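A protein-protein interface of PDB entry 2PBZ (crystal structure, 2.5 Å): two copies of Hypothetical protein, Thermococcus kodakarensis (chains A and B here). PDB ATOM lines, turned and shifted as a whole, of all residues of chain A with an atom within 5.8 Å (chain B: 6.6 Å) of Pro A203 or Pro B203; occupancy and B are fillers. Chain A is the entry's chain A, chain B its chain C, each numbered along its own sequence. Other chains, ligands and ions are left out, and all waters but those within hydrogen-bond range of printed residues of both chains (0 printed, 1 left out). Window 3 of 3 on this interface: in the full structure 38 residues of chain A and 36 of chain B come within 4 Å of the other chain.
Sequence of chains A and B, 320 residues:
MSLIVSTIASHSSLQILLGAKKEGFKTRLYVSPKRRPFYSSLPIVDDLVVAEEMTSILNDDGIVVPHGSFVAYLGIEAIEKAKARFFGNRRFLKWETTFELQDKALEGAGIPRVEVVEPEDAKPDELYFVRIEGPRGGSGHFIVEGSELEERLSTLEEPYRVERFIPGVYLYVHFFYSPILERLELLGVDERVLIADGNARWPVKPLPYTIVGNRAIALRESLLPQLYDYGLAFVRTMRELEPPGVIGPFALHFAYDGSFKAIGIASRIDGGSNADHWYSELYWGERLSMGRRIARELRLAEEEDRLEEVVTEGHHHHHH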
ATOM      1  N   GLY A 198     -12.365  -2.782  14.389  1.00  0.00           N
ATOM      2  CA  GLY A 198     -11.630  -2.280  13.236  1.00  0.00           C
ATOM      3  C   GLY A 198     -11.814  -3.286  12.108  1.00  0.00           C
ATOM      4  O   GLY A 198     -11.270  -3.091  11.029  1.00  0.00           O
ATOM      5  N   ASN A 199     -12.545  -4.380  12.365  1.00  0.00           N
ATOM      6  CA  ASN A 199     -12.861  -5.366  11.341  1.00  0.00           C
ATOM      7  C   ASN A 199     -14.318  -5.149  11.137  1.00  0.00           C
ATOM      8  O   ASN A 199     -14.865  -5.513  10.108  1.00  0.00           O
ATOM      9  CB  ASN A 199     -12.651  -6.816  11.802  1.00  0.00           C
ATOM     10  CG  ASN A 199     -11.227  -7.290  11.602  1.00  0.00           C
ATOM     11  OD1 ASN A 199     -10.396  -6.575  11.029  1.00  0.00           O
ATOM     12  ND2 ASN A 199     -10.933  -8.487  12.074  1.00  0.00           N
ATOM     13  N   ALA A 200     -14.951  -4.561  12.142  1.00  0.00           N
ATOM     14  CA  ALA A 200     -16.368  -4.280  12.058  1.00  0.00           C
ATOM     15  C   ALA A 200     -16.576  -3.289  10.920  1.00  0.00           C
ATOM     16  O   ALA A 200     -17.481  -3.445  10.099  1.00  0.00           O
ATOM     17  CB  ALA A 200     -16.852  -3.687  13.355  1.00  0.00           C
ATOM     18  N   ARG A 201     -15.716  -2.270  10.889  1.00  0.00           N
ATOM     19  CA  ARG A 201     -15.769  -1.232   9.868  1.00  0.00           C
ATOM     20  C   ARG A 201     -15.331  -1.830   8.534  1.00  0.00           C
ATOM     21  O   ARG A 201     -15.995  -1.665   7.515  1.00  0.00           O
ATOM     22  CB  ARG A 201     -14.822  -0.097  10.224  1.00  0.00           C
ATOM     23  CG  ARG A 201     -14.887   0.371  11.659  1.00  0.00           C
ATOM     24  CD  ARG A 201     -16.037   1.315  11.946  1.00  0.00           C
ATOM     25  NE  ARG A 201     -15.689   2.112  13.108  1.00  0.00           N
ATOM     26  CZ  ARG A 201     -16.553   2.621  13.978  1.00  0.00           C
ATOM     27  NH1 ARG A 201     -17.872   2.425  13.837  1.00  0.00           N
ATOM     28  NH2 ARG A 201     -16.089   3.329  15.001  1.00  0.00           N
ATOM     29  N   TRP A 202     -14.191  -2.512   8.556  1.00  0.00           N
ATOM     30  CA  TRP A 202     -13.654  -3.160   7.372  1.00  0.00           C
ATOM     31  C   TRP A 202     -12.775  -4.315   7.800  1.00  0.00           C
ATOM     32  O   TRP A 202     -11.686  -4.113   8.331  1.00  0.00           O
ATOM     33  CB  TRP A 202     -12.826  -2.194   6.519  1.00  0.00           C
ATOM     34  CG  TRP A 202     -12.412  -2.827   5.211  1.00  0.00           C
ATOM     35  CD1 TRP A 202     -11.140  -3.048   4.765  1.00  0.00           C
ATOM     36  CD2 TRP A 202     -13.287  -3.420   4.229  1.00  0.00           C
ATOM     37  NE1 TRP A 202     -11.162  -3.743   3.577  1.00  0.00           N
ATOM     38  CE2 TRP A 202     -12.468  -3.989   3.227  1.00  0.00           C
ATOM     39  CE3 TRP A 202     -14.682  -3.530   4.104  1.00  0.00           C
ATOM     40  CZ2 TRP A 202     -13.004  -4.663   2.108  1.00  0.00           C
ATOM     41  CZ3 TRP A 202     -15.214  -4.201   2.989  1.00  0.00           C
ATOM     42  CH2 TRP A 202     -14.373  -4.756   2.009  1.00  0.00           C
ATOM     43  N   PRO A 203     -13.235  -5.552   7.562  1.00  0.00           N
ATOM     44  CA  PRO A 203     -12.485  -6.758   7.929  1.00  0.00           C
ATOM     45  C   PRO A 203     -11.158  -6.860   7.178  1.00  0.00           C
ATOM     46  O   PRO A 203     -11.093  -6.599   5.974  1.00  0.00           O
ATOM     47  CB  PRO A 203     -13.457  -7.887   7.592  1.00  0.00           C
ATOM     48  CG  PRO A 203     -14.255  -7.319   6.453  1.00  0.00           C
ATOM     49  CD  PRO A 203     -14.503  -5.898   6.897  1.00  0.00           C
ATOM     50  N   VAL A 204     -10.098  -7.219   7.894  1.00  0.00           N
ATOM     51  CA  VAL A 204      -8.775  -7.342   7.291  1.00  0.00           C
ATOM     52  C   VAL A 204      -8.156  -8.718   7.541  1.00  0.00           C
ATOM     53  O   VAL A 204      -7.954  -9.507   6.612  1.00  0.00           O
ATOM     54  CB  VAL A 204      -7.811  -6.278   7.850  1.00  0.00           C
ATOM     55  CG1 VAL A 204      -6.514  -6.276   7.036  1.00  0.00           C
ATOM     56  CG2 VAL A 204      -8.482  -4.910   7.841  1.00  0.00           C
ATOM     57  N   LYS A 205      -7.846  -8.992   8.805  1.00  0.00           N
ATOM     58  CA  LYS A 205      -7.251 -10.263   9.212  1.00  0.00           C
ATOM     59  C   LYS A 205      -7.630 -10.606  10.650  1.00  0.00           C
ATOM     60  O   LYS A 205      -8.045  -9.734  11.418  1.00  0.00           O
ATOM     61  CB  LYS A 205      -5.719 -10.194   9.119  1.00  0.00           C
ATOM     62  CG  LYS A 205      -5.105  -9.011   9.883  1.00  0.00           C
ATOM     63  CD  LYS A 205      -3.572  -9.026   9.878  1.00  0.00           C
ATOM     64  CE  LYS A 205      -3.032 -10.221  10.666  1.00  0.00           C
ATOM     65  NZ  LYS A 205      -1.550 -10.191  10.885  1.00  0.00           N
ATOM     66  N   GLY B 198     -20.198 -11.557  16.059  1.00  0.00           N
ATOM     67  CA  GLY B 198     -19.247 -12.653  15.899  1.00  0.00           C
ATOM     68  C   GLY B 198     -18.746 -12.610  14.458  1.00  0.00           C
ATOM     69  O   GLY B 198     -17.922 -13.448  14.077  1.00  0.00           O
ATOM     70  N   ASN B 199     -19.264 -11.666  13.642  1.00  0.00           N
ATOM     71  CA  ASN B 199     -18.801 -11.477  12.266  1.00  0.00           C
ATOM     72  C   ASN B 199     -18.064 -10.186  12.362  1.00  0.00           C
ATOM     73  O   ASN B 199     -17.216  -9.887  11.538  1.00  0.00           O
ATOM     74  CB  ASN B 199     -19.941 -11.313  11.259  1.00  0.00           C
ATOM     75  CG  ASN B 199     -20.448 -12.642  10.727  1.00  0.00           C
ATOM     76  OD1 ASN B 199     -19.876 -13.697  11.016  1.00  0.00           O
ATOM     77  ND2 ASN B 199     -21.516 -12.600   9.947  1.00  0.00           N
ATOM     78  N   ALA B 200     -18.403  -9.412  13.378  1.00  0.00           N
ATOM     79  CA  ALA B 200     -17.734  -8.145  13.587  1.00  0.00           C
ATOM     80  C   ALA B 200     -16.259  -8.413  13.875  1.00  0.00           C
ATOM     81  O   ALA B 200     -15.383  -7.721  13.352  1.00  0.00           O
ATOM     82  CB  ALA B 200     -18.368  -7.413  14.748  1.00  0.00           C
ATOM     83  N   ARG B 201     -16.010  -9.426  14.708  1.00  0.00           N
ATOM     84  CA  ARG B 201     -14.656  -9.827  15.098  1.00  0.00           C
ATOM     85  C   ARG B 201     -13.992 -10.497  13.905  1.00  0.00           C
ATOM     86  O   ARG B 201     -12.867 -10.181  13.547  1.00  0.00           O
ATOM     87  CB  ARG B 201     -14.705 -10.834  16.246  1.00  0.00           C
ATOM     88  CG  ARG B 201     -15.626 -10.476  17.388  1.00  0.00           C
ATOM     89  CD  ARG B 201     -15.046  -9.467  18.357  1.00  0.00           C
ATOM     90  NE  ARG B 201     -15.736  -9.611  19.632  1.00  0.00           N
ATOM     91  CZ  ARG B 201     -15.933  -8.633  20.503  1.00  0.00           C
ATOM     92  NH1 ARG B 201     -15.482  -7.403  20.238  1.00  0.00           N
ATOM     93  NH2 ARG B 201     -16.579  -8.888  21.638  1.00  0.00           N
ATOM     94  N   TRP B 202     -14.708 -11.444  13.310  1.00  0.00           N
ATOM     95  CA  TRP B 202     -14.225 -12.176  12.155  1.00  0.00           C
ATOM     96  C   TRP B 202     -15.410 -12.706  11.376  1.00  0.00           C
ATOM     97  O   TRP B 202     -16.093 -13.634  11.819  1.00  0.00           O
ATOM     98  CB  TRP B 202     -13.334 -13.360  12.553  1.00  0.00           C
ATOM     99  CG  TRP B 202     -12.713 -14.009  11.329  1.00  0.00           C
ATOM    100  CD1 TRP B 202     -12.876 -15.298  10.901  1.00  0.00           C
ATOM    101  CD2 TRP B 202     -11.906 -13.356  10.335  1.00  0.00           C
ATOM    102  NE1 TRP B 202     -12.228 -15.485   9.698  1.00  0.00           N
ATOM    103  CE2 TRP B 202     -11.625 -14.311   9.329  1.00  0.00           C
ATOM    104  CE3 TRP B 202     -11.397 -12.054  10.196  1.00  0.00           C
ATOM    105  CZ2 TRP B 202     -10.851 -14.007   8.193  1.00  0.00           C
ATOM    106  CZ3 TRP B 202     -10.627 -11.748   9.063  1.00  0.00           C
ATOM    107  CH2 TRP B 202     -10.363 -12.729   8.077  1.00  0.00           C
ATOM    108  N   PRO B 203     -15.667 -12.118  10.195  1.00  0.00           N
ATOM    109  CA  PRO B 203     -16.777 -12.523   9.325  1.00  0.00           C
ATOM    110  C   PRO B 203     -16.626 -13.964   8.841  1.00  0.00           C
ATOM    111  O   PRO B 203     -15.538 -14.380   8.449  1.00  0.00           O
ATOM    112  CB  PRO B 203     -16.718 -11.491   8.194  1.00  0.00           C
ATOM    113  CG  PRO B 203     -15.272 -11.137   8.124  1.00  0.00           C
ATOM    114  CD  PRO B 203     -14.888 -11.024   9.582  1.00  0.00           C
ATOM    115  N   VAL B 204     -17.718 -14.722   8.895  1.00  0.00           N
ATOM    116  CA  VAL B 204     -17.726 -16.122   8.472  1.00  0.00           C
ATOM    117  C   VAL B 204     -18.796 -16.396   7.407  1.00  0.00           C
ATOM    118  O   VAL B 204     -18.477 -16.704   6.257  1.00  0.00           O
ATOM    119  CB  VAL B 204     -17.999 -17.057   9.661  1.00  0.00           C
ATOM    120  CG1 VAL B 204     -17.763 -18.512   9.240  1.00  0.00           C
ATOM    121  CG2 VAL B 204     -17.136 -16.655  10.843  1.00  0.00           C
ATOM    122  N   LYS B 205     -20.063 -16.297   7.798  1.00  0.00           N
ATOM    123  CA  LYS B 205     -21.178 -16.533   6.884  1.00  0.00           C
ATOM    124  C   LYS B 205     -22.384 -15.711   7.319  1.00  0.00           C
ATOM    125  O   LYS B 205     -22.454 -15.232   8.458  1.00  0.00           O
ATOM    126  CB  LYS B 205     -21.570 -18.020   6.881  1.00  0.00           C
ATOM    127  CG  LYS B 205     -21.806 -18.619   8.288  1.00  0.00           C
ATOM    128  CD  LYS B 205     -22.309 -20.084   8.252  1.00  0.00           C
ATOM    129  CE  LYS B 205     -23.740 -20.155   7.691  1.00  0.00           C
ATOM    130  NZ  LYS B 205     -24.408 -21.500   7.786  1.00  0.00           N
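The backbone carbonyl oxygen (O) of Arg B201 sits at hydrogen-bond distance from the side-chain amide nitrogen (ND2) of Asn A199 (3.0 Å). The backbone carbonyl oxygen of Ala B200 sits at hydrogen-bond distance from the backbone NH of Ala A200 (3.4 Å).
The backbone NH of Val A204 is in hydrogen-bond range of the side-chain amide oxygen of Asn A199, 3.2 Å away. ND2 of Asn A199 lies within hydrogen-bond range of O of Lys A205.
Among the printed residues, pairs that only touch across the chains: Asn A199 with Ala B200 (3.3 Å), Pro A203 with Pro B203 (3.8 Å) and Lys A205 with Trp B202 (3.6 Å).
Pro A203 touches just one residue of chain B: Pro B203 (3.8 Å). Of the printed residues of chain A, Pro B203 touches Pro A203. Of the printed residues of chain B, Lys A205 touches Trp B202 (3.6 Å). Printed residues of chain B within 4 Å of Asn A199: Ala B200 and Arg B201. Arg A201 touches none of the printed residues of chain B. The nearest residue of chain B that does not touch Pro A203 is Trp B202 (5.0 Å). The nearest residue of chain A that does not touch Pro B203 is Asn A199 (5.3 Å).
Hydrophobic or aromatic side chains of chain A within 4 Å of the printed part of chain B: Pro A203. Of the 8 printed residues of chain B, 4 touch a printed residue of chain A. Hydrophobic or aromatic side chains of chain B that line the printed part of chain A: Trp B202 and Pro B203. Among the printed residues, 5 pairs touch across the chains. Among the printed residues, no Asp or Glu carboxylate lies within 4 Å of a Lys or Arg side-chain nitrogen of the other chain.
Asn A199 touches Arg B201, but with the chains exchanged Arg A201 does not touch Asn B199 (7.8 Å). Ala A200 touches its own counterpart, Ala B200. Pro B203 touches its own counterpart, Pro A203. Lys A205 touches Trp B202, but with the chains exchanged Trp A202 does not touch Lys B205 (13.9 Å). Positions printed for both chains: 198, 199, 200, 201, 202, 203, 204 and 205.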
